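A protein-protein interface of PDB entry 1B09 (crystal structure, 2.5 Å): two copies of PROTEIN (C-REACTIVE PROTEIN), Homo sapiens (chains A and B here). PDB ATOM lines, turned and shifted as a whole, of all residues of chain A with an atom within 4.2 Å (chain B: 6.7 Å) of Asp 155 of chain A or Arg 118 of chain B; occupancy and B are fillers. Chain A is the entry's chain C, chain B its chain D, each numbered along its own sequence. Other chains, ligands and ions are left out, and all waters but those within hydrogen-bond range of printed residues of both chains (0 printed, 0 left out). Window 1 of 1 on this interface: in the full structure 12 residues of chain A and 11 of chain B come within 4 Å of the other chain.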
ATOM      1  N   PHE A   9      -6.419 -19.382  -2.471  1.00  0.00           N
ATOM      2  CA  PHE A   9      -5.809 -18.231  -1.805  1.00  0.00           C
ATOM      3  C   PHE A   9      -5.511 -18.504  -0.351  1.00  0.00           C
ATOM      4  O   PHE A   9      -6.428 -18.889   0.431  1.00  0.00           O
ATOM      5  CB  PHE A   9      -6.796 -17.063  -1.895  1.00  0.00           C
ATOM      6  CG  PHE A   9      -6.819 -16.494  -3.294  1.00  0.00           C
ATOM      7  CD1 PHE A   9      -5.634 -16.148  -3.936  1.00  0.00           C
ATOM      8  CD2 PHE A   9      -8.038 -16.274  -3.909  1.00  0.00           C
ATOM      9  CE1 PHE A   9      -5.681 -15.572  -5.200  1.00  0.00           C
ATOM     10  CE2 PHE A   9      -8.076 -15.699  -5.172  1.00  0.00           C
ATOM     11  CZ  PHE A   9      -6.900 -15.348  -5.822  1.00  0.00           C
ATOM     12  N   VAL A  10      -4.228 -18.348   0.041  1.00  0.00           N
ATOM     13  CA  VAL A  10      -3.887 -18.663   1.429  1.00  0.00           C
ATOM     14  C   VAL A  10      -3.483 -17.442   2.276  1.00  0.00           C
ATOM     15  O   VAL A  10      -2.494 -16.729   1.976  1.00  0.00           O
ATOM     16  CB  VAL A  10      -2.746 -19.695   1.417  1.00  0.00           C
ATOM     17  CG1 VAL A  10      -1.841 -19.487   0.213  1.00  0.00           C
ATOM     18  CG2 VAL A  10      -1.905 -19.555   2.672  1.00  0.00           C
ATOM     19  N   PHE A  39     -13.591 -23.367   2.131  1.00  0.00           N
ATOM     20  CA  PHE A  39     -12.734 -22.684   3.111  1.00  0.00           C
ATOM     21  C   PHE A  39     -12.379 -23.531   4.317  1.00  0.00           C
ATOM     22  O   PHE A  39     -13.196 -24.407   4.746  1.00  0.00           O
ATOM     23  CB  PHE A  39     -13.458 -21.402   3.569  1.00  0.00           C
ATOM     24  CG  PHE A  39     -14.517 -21.734   4.602  1.00  0.00           C
ATOM     25  CD1 PHE A  39     -14.173 -21.783   5.946  1.00  0.00           C
ATOM     26  CD2 PHE A  39     -15.829 -21.961   4.206  1.00  0.00           C
ATOM     27  CE1 PHE A  39     -15.155 -22.060   6.895  1.00  0.00           C
ATOM     28  CE2 PHE A  39     -16.800 -22.236   5.160  1.00  0.00           C
ATOM     29  CZ  PHE A  39     -16.467 -22.288   6.508  1.00  0.00           C
ATOM     30  N   TYR A  40     -11.092 -23.309   4.704  1.00  0.00           N
ATOM     31  CA  TYR A  40     -10.453 -24.109   5.769  1.00  0.00           C
ATOM     32  C   TYR A  40      -9.704 -23.232   6.766  1.00  0.00           C
ATOM     33  O   TYR A  40      -8.695 -22.561   6.417  1.00  0.00           O
ATOM     34  CB  TYR A  40      -9.469 -25.070   5.069  1.00  0.00           C
ATOM     35  CG  TYR A  40      -8.817 -26.016   6.070  1.00  0.00           C
ATOM     36  CD1 TYR A  40      -9.541 -26.527   7.151  1.00  0.00           C
ATOM     37  CD2 TYR A  40      -7.491 -26.415   5.884  1.00  0.00           C
ATOM     38  CE1 TYR A  40      -8.937 -27.423   8.028  1.00  0.00           C
ATOM     39  CE2 TYR A  40      -6.892 -27.308   6.759  1.00  0.00           C
ATOM     40  CZ  TYR A  40      -7.609 -27.813   7.827  1.00  0.00           C
ATOM     41  OH  TYR A  40      -7.036 -28.732   8.679  1.00  0.00           O
ATOM     42  N   GLY A 154      -6.356 -18.662   7.027  1.00  0.00           N
ATOM     43  CA  GLY A 154      -6.541 -19.974   6.428  1.00  0.00           C
ATOM     44  C   GLY A 154      -6.632 -19.909   4.921  1.00  0.00           C
ATOM     45  O   GLY A 154      -6.194 -18.911   4.276  1.00  0.00           O
ATOM     46  N   ASP A 155      -7.159 -20.994   4.326  1.00  0.00           N
ATOM     47  CA  ASP A 155      -7.338 -21.018   2.878  1.00  0.00           C
ATOM     48  C   ASP A 155      -8.772 -20.779   2.459  1.00  0.00           C
ATOM     49  O   ASP A 155      -9.720 -21.132   3.194  1.00  0.00           O
ATOM     50  CB  ASP A 155      -6.902 -22.395   2.367  1.00  0.00           C
ATOM     51  CG  ASP A 155      -5.413 -22.528   2.553  1.00  0.00           C
ATOM     52  OD1 ASP A 155      -4.917 -22.085   3.587  1.00  0.00           O
ATOM     53  OD2 ASP A 155      -4.765 -23.059   1.661  1.00  0.00           O
ATOM     54  N   ILE A 156      -8.947 -20.132   1.291  1.00  0.00           N
ATOM     55  CA  ILE A 156     -10.267 -20.112   0.679  1.00  0.00           C
ATOM     56  C   ILE A 156     -10.192 -20.181  -0.839  1.00  0.00           C
ATOM     57  O   ILE A 156      -9.231 -19.673  -1.459  1.00  0.00           O
ATOM     58  CB  ILE A 156     -10.996 -18.821   1.121  1.00  0.00           C
ATOM     59  CG1 ILE A 156     -12.290 -18.638   0.315  1.00  0.00           C
ATOM     60  CG2 ILE A 156     -10.132 -17.588   0.870  1.00  0.00           C
ATOM     61  CD1 ILE A 156     -13.393 -17.979   1.155  1.00  0.00           C
ATOM     62  N   LYS A 201      -1.676 -21.065  -3.672  1.00  0.00           N
ATOM     63  CA  LYS A 201      -1.108 -22.409  -3.570  1.00  0.00           C
ATOM     64  C   LYS A 201      -2.084 -23.507  -3.927  1.00  0.00           C
ATOM     65  O   LYS A 201      -3.325 -23.287  -4.007  1.00  0.00           O
ATOM     66  CB  LYS A 201      -0.664 -22.597  -2.130  1.00  0.00           C
ATOM     67  CG  LYS A 201       0.552 -21.740  -1.781  1.00  0.00           C
ATOM     68  CD  LYS A 201       1.875 -22.418  -2.146  1.00  0.00           C
ATOM     69  CE  LYS A 201       3.089 -21.584  -1.737  1.00  0.00           C
ATOM     70  NZ  LYS A 201       4.309 -22.350  -1.961  1.00  0.00           N
ATOM     71  N   PRO A 202      -1.533 -24.712  -4.179  1.00  0.00           N
ATOM     72  CA  PRO A 202      -2.409 -25.845  -4.488  1.00  0.00           C
ATOM     73  C   PRO A 202      -3.337 -26.150  -3.328  1.00  0.00           C
ATOM     74  O   PRO A 202      -2.992 -26.032  -2.154  1.00  0.00           O
ATOM     75  CB  PRO A 202      -1.524 -27.052  -4.788  1.00  0.00           C
ATOM     76  CG  PRO A 202      -0.137 -26.534  -5.157  1.00  0.00           C
ATOM     77  CD  PRO A 202      -0.156 -25.060  -4.517  1.00  0.00           C
ATOM     78  N   LEU A 204      -5.765 -27.786  -0.468  1.00  0.00           N
ATOM     79  CA  LEU A 204      -5.656 -28.932   0.441  1.00  0.00           C
ATOM     80  C   LEU A 204      -6.874 -29.835   0.420  1.00  0.00           C
ATOM     81  O   LEU A 204      -6.826 -31.017   0.877  1.00  0.00           O
ATOM     82  CB  LEU A 204      -5.468 -28.407   1.864  1.00  0.00           C
ATOM     83  CG  LEU A 204      -4.217 -27.548   2.031  1.00  0.00           C
ATOM     84  CD1 LEU A 204      -4.091 -26.965   3.444  1.00  0.00           C
ATOM     85  CD2 LEU A 204      -2.933 -28.339   1.772  1.00  0.00           C
ATOM     86  N   TRP A 205      -8.007 -29.288  -0.040  1.00  0.00           N
ATOM     87  CA  TRP A 205      -9.138 -30.154  -0.221  1.00  0.00           C
ATOM     88  C   TRP A 205      -9.177 -30.785  -1.592  1.00  0.00           C
ATOM     89  O   TRP A 205      -8.464 -30.346  -2.530  1.00  0.00           O
ATOM     90  CB  TRP A 205     -10.447 -29.355   0.031  1.00  0.00           C
ATOM     91  CG  TRP A 205     -10.503 -28.101  -0.802  1.00  0.00           C
ATOM     92  CD1 TRP A 205     -11.015 -27.977  -2.110  1.00  0.00           C
ATOM     93  CD2 TRP A 205     -10.118 -26.768  -0.379  1.00  0.00           C
ATOM     94  NE1 TRP A 205     -10.984 -26.694  -2.560  1.00  0.00           N
ATOM     95  CE2 TRP A 205     -10.416 -25.892  -1.453  1.00  0.00           C
ATOM     96  CE3 TRP A 205      -9.562 -26.256   0.786  1.00  0.00           C
ATOM     97  CZ2 TRP A 205     -10.149 -24.536  -1.331  1.00  0.00           C
ATOM     98  CZ3 TRP A 205      -9.305 -24.907   0.912  1.00  0.00           C
ATOM     99  CH2 TRP A 205      -9.593 -24.041  -0.161  1.00  0.00           C
ATOM    100  N   PHE B  84       1.310 -26.581  16.477  1.00  0.00           N
ATOM    101  CA  PHE B  84       0.027 -27.202  16.097  1.00  0.00           C
ATOM    102  C   PHE B  84      -0.582 -27.994  17.231  1.00  0.00           C
ATOM    103  O   PHE B  84      -0.105 -29.115  17.578  1.00  0.00           O
ATOM    104  CB  PHE B  84       0.250 -28.140  14.891  1.00  0.00           C
ATOM    105  CG  PHE B  84       0.910 -27.406  13.743  1.00  0.00           C
ATOM    106  CD1 PHE B  84       0.123 -26.753  12.798  1.00  0.00           C
ATOM    107  CD2 PHE B  84       2.293 -27.398  13.626  1.00  0.00           C
ATOM    108  CE1 PHE B  84       0.736 -26.093  11.732  1.00  0.00           C
ATOM    109  CE2 PHE B  84       2.895 -26.739  12.563  1.00  0.00           C
ATOM    110  CZ  PHE B  84       2.122 -26.086  11.611  1.00  0.00           C
ATOM    111  N   ILE B 106       5.816 -20.199   4.117  1.00  0.00           N
ATOM    112  CA  ILE B 106       4.689 -21.019   4.513  1.00  0.00           C
ATOM    113  C   ILE B 106       5.125 -22.396   4.967  1.00  0.00           C
ATOM    114  O   ILE B 106       5.932 -23.070   4.302  1.00  0.00           O
ATOM    115  CB  ILE B 106       3.762 -21.166   3.310  1.00  0.00           C
ATOM    116  CG1 ILE B 106       3.113 -19.811   2.961  1.00  0.00           C
ATOM    117  CG2 ILE B 106       2.647 -22.163   3.625  1.00  0.00           C
ATOM    118  CD1 ILE B 106       1.854 -19.968   2.102  1.00  0.00           C
ATOM    119  N   VAL B 107       4.617 -22.826   6.135  1.00  0.00           N
ATOM    120  CA  VAL B 107       4.838 -24.215   6.505  1.00  0.00           C
ATOM    121  C   VAL B 107       3.568 -25.046   6.508  1.00  0.00           C
ATOM    122  O   VAL B 107       2.486 -24.600   6.977  1.00  0.00           O
ATOM    123  CB  VAL B 107       5.507 -24.274   7.892  1.00  0.00           C
ATOM    124  CG1 VAL B 107       6.468 -23.097   8.065  1.00  0.00           C
ATOM    125  CG2 VAL B 107       4.463 -24.256   9.005  1.00  0.00           C
ATOM    126  N   GLU B 108       3.683 -26.263   5.927  1.00  0.00           N
ATOM    127  CA  GLU B 108       2.584 -27.233   5.976  1.00  0.00           C
ATOM    128  C   GLU B 108       2.867 -28.359   6.943  1.00  0.00           C
ATOM    129  O   GLU B 108       4.042 -28.812   7.078  1.00  0.00           O
ATOM    130  CB  GLU B 108       2.436 -27.801   4.562  1.00  0.00           C
ATOM    131  CG  GLU B 108       1.329 -27.118   3.756  1.00  0.00           C
ATOM    132  CD  GLU B 108       1.517 -27.474   2.301  1.00  0.00           C
ATOM    133  OE1 GLU B 108       1.975 -28.574   2.019  1.00  0.00           O
ATOM    134  OE2 GLU B 108       1.206 -26.641   1.454  1.00  0.00           O
ATOM    135  N   PHE B 109       1.813 -28.820   7.665  1.00  0.00           N
ATOM    136  CA  PHE B 109       2.029 -29.925   8.626  1.00  0.00           C
ATOM    137  C   PHE B 109       1.019 -31.060   8.486  1.00  0.00           C
ATOM    138  O   PHE B 109      -0.191 -30.919   8.862  1.00  0.00           O
ATOM    139  CB  PHE B 109       1.957 -29.312  10.050  1.00  0.00           C
ATOM    140  CG  PHE B 109       2.692 -30.193  11.060  1.00  0.00           C
ATOM    141  CD1 PHE B 109       4.080 -30.153  11.160  1.00  0.00           C
ATOM    142  CD2 PHE B 109       1.956 -31.007  11.907  1.00  0.00           C
ATOM    143  CE1 PHE B 109       4.727 -30.941  12.116  1.00  0.00           C
ATOM    144  CE2 PHE B 109       2.611 -31.788  12.859  1.00  0.00           C
ATOM    145  CZ  PHE B 109       3.995 -31.763  12.959  1.00  0.00           C
ATOM    146  N   TRP B 110       1.488 -32.196   7.899  1.00  0.00           N
ATOM    147  CA  TRP B 110       0.575 -33.302   7.595  1.00  0.00           C
ATOM    148  C   TRP B 110       0.597 -34.412   8.647  1.00  0.00           C
ATOM    149  O   TRP B 110       1.676 -34.981   8.969  1.00  0.00           O
ATOM    150  CB  TRP B 110       1.006 -33.916   6.259  1.00  0.00           C
ATOM    151  CG  TRP B 110       0.802 -32.941   5.121  1.00  0.00           C
ATOM    152  CD1 TRP B 110       1.727 -31.975   4.666  1.00  0.00           C
ATOM    153  CD2 TRP B 110      -0.322 -32.896   4.196  1.00  0.00           C
ATOM    154  NE1 TRP B 110       1.298 -31.325   3.547  1.00  0.00           N
ATOM    155  CE2 TRP B 110      -0.019 -31.909   3.217  1.00  0.00           C
ATOM    156  CE3 TRP B 110      -1.520 -33.591   4.107  1.00  0.00           C
ATOM    157  CZ2 TRP B 110      -0.914 -31.652   2.191  1.00  0.00           C
ATOM    158  CZ3 TRP B 110      -2.408 -33.336   3.078  1.00  0.00           C
ATOM    159  CH2 TRP B 110      -2.100 -32.352   2.116  1.00  0.00           C
ATOM    160  N   ARG B 116      -2.895 -29.937   8.139  1.00  0.00           N
ATOM    161  CA  ARG B 116      -3.333 -28.799   8.933  1.00  0.00           C
ATOM    162  C   ARG B 116      -3.304 -27.498   8.157  1.00  0.00           C
ATOM    163  O   ARG B 116      -2.513 -27.331   7.169  1.00  0.00           O
ATOM    164  CB  ARG B 116      -2.392 -28.665  10.164  1.00  0.00           C
ATOM    165  CG  ARG B 116      -2.201 -29.982  10.943  1.00  0.00           C
ATOM    166  CD  ARG B 116      -3.358 -30.281  11.907  1.00  0.00           C
ATOM    167  NE  ARG B 116      -3.575 -29.161  12.831  1.00  0.00           N
ATOM    168  CZ  ARG B 116      -3.421 -29.399  14.157  1.00  0.00           C
ATOM    169  NH1 ARG B 116      -3.048 -30.597  14.588  1.00  0.00           N
ATOM    170  NH2 ARG B 116      -3.664 -28.419  15.038  1.00  0.00           N
ATOM    171  N   VAL B 117      -4.183 -26.583   8.561  1.00  0.00           N
ATOM    172  CA  VAL B 117      -4.065 -25.214   8.131  1.00  0.00           C
ATOM    173  C   VAL B 117      -2.609 -24.766   7.964  1.00  0.00           C
ATOM    174  O   VAL B 117      -1.679 -25.285   8.638  1.00  0.00           O
ATOM    175  CB  VAL B 117      -4.745 -24.360   9.183  1.00  0.00           C
ATOM    176  CG1 VAL B 117      -4.530 -22.885   8.904  1.00  0.00           C
ATOM    177  CG2 VAL B 117      -6.237 -24.647   9.186  1.00  0.00           C
ATOM    178  N   ARG B 118      -2.401 -23.817   7.025  1.00  0.00           N
ATOM    179  CA  ARG B 118      -1.047 -23.319   6.769  1.00  0.00           C
ATOM    180  C   ARG B 118      -0.626 -22.225   7.727  1.00  0.00           C
ATOM    181  O   ARG B 118      -1.490 -21.476   8.286  1.00  0.00           O
ATOM    182  CB  ARG B 118      -1.028 -22.781   5.330  1.00  0.00           C
ATOM    183  CG  ARG B 118      -1.573 -23.808   4.324  1.00  0.00           C
ATOM    184  CD  ARG B 118      -0.552 -24.146   3.228  1.00  0.00           C
ATOM    185  NE  ARG B 118      -1.173 -25.005   2.214  1.00  0.00           N
ATOM    186  CZ  ARG B 118      -1.447 -24.457   1.017  1.00  0.00           C
ATOM    187  NH1 ARG B 118      -1.164 -23.188   0.777  1.00  0.00           N
ATOM    188  NH2 ARG B 118      -2.024 -25.201   0.079  1.00  0.00           N
ATOM    189  N   LYS B 119       0.686 -22.125   7.962  1.00  0.00           N
ATOM    190  CA  LYS B 119       1.167 -21.045   8.796  1.00  0.00           C
ATOM    191  C   LYS B 119       2.439 -20.414   8.272  1.00  0.00           C
ATOM    192  O   LYS B 119       3.086 -20.930   7.313  1.00  0.00           O
ATOM    193  CB  LYS B 119       1.397 -21.615  10.195  1.00  0.00           C
ATOM    194  CG  LYS B 119       0.110 -22.230  10.780  1.00  0.00           C
ATOM    195  CD  LYS B 119       0.231 -22.556  12.269  1.00  0.00           C
ATOM    196  CE  LYS B 119      -1.058 -23.153  12.847  1.00  0.00           C
ATOM    197  NZ  LYS B 119      -0.997 -23.121  14.309  1.00  0.00           N
ATOM    198  N   SER B 120       2.803 -19.251   8.856  1.00  0.00           N
ATOM    199  CA  SER B 120       3.997 -18.540   8.368  1.00  0.00           C
ATOM    200  C   SER B 120       5.163 -18.649   9.314  1.00  0.00           C
ATOM    201  O   SER B 120       4.998 -18.603  10.558  1.00  0.00           O
ATOM    202  CB  SER B 120       3.607 -17.069   8.188  1.00  0.00           C
ATOM    203  OG  SER B 120       4.572 -16.423   7.349  1.00  0.00           O
ATOM    204  N   PRO B 168       0.357 -32.011  -2.536  1.00  0.00           N
ATOM    205  CA  PRO B 168      -0.596 -32.861  -1.811  1.00  0.00           C
ATOM    206  C   PRO B 168      -0.726 -34.259  -2.411  1.00  0.00           C
ATOM    207  O   PRO B 168      -1.036 -35.240  -1.731  1.00  0.00           O
ATOM    208  CB  PRO B 168      -1.957 -32.166  -1.818  1.00  0.00           C
ATOM    209  CG  PRO B 168      -1.718 -30.691  -2.098  1.00  0.00           C
ATOM    210  CD  PRO B 168      -0.307 -30.747  -2.863  1.00  0.00           C
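Of the printed residues of chain B, Tyr 40 of chain A touches Arg 116 (3.7 Å) and Val 117 (3.3 Å).
Asp 155 of chain A touches just one residue of chain B: Arg 118.
Ile 156 of chain A touches none of the printed residues of chain B.
Of the printed residues of chain B, Pro 202 of chain A touches Arg 118 (2.6 Å).
Of the printed residues of chain A, Ile 106 of chain B touches Val 10.
Val 107 of chain B touches none of the printed residues of chain A.
Of the printed residues of chain A, Arg 116 of chain B touches Tyr 40.
Arg 118 of chain B touches five residues of chain A.
The nearest printed residue of chain A that does not touch Trp 110 of chain B is Trp 205 of chain A (7.0 Å).
The guanidinium group (NH2) of Arg 118 of chain B lies within hydrogen-bond range of the backbone carbonyl oxygen (O) of Pro 202 of chain A, 2.6 Å away.
The side-chain carboxylate of Asp 155 of chain A lies within salt-bridge range of the guanidinium group of Arg 118 of chain B (3.7 Å).
No position is printed for both chains.
Of the 9 pairs that touch across the chains among the printed residues, none has its exchanged pair printed and touching as well.
CD1 of Ile 106 of chain B touches CG2 of Val 10 of chain A, 3.8 Å away.
Val 10 of chain A touches Arg 118 of chain B (CG1 to NH1, 3.8 Å).
Tyr 40 of chain A touches Arg 116 of chain B.
Tyr 40 of chain A touches Val 117 of chain B.
Arg 118 of chain B touches Lys 201 of chain A.
CZ2 of Trp 110 of chain B touches CD2 of Leu 204 of chain A, at 3.9 Å.
Leu 204 of chain A touches Arg 118 of chain B.
Hydrophobic or aromatic side chains of chain B that line the printed part of chain A: Ile 106, Trp 110 and Val 117.
Along chain A the printed residues that touch a printed residue of chain B span positions 10 to 204.
The indole nitrogen (NE1) of Trp 110 of chain B is in hydrogen-bond range of the side-chain carboxylate (OE1) of Glu 108 of chain B (3.2 Å).
The backbone NH (N) of Arg 116 of chain B sits at hydrogen-bond distance from the backbone carbonyl oxygen (O) of Phe 109 of chain B (3.0 Å).
O of Asp 155 of chain A lies within hydrogen-bond range of N of Tyr 40 of chain A, 3.0 Å away.
OE2 of Glu 108 of chain B is in salt-bridge range of NE of Arg 118 of chain B (3.0 Å).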
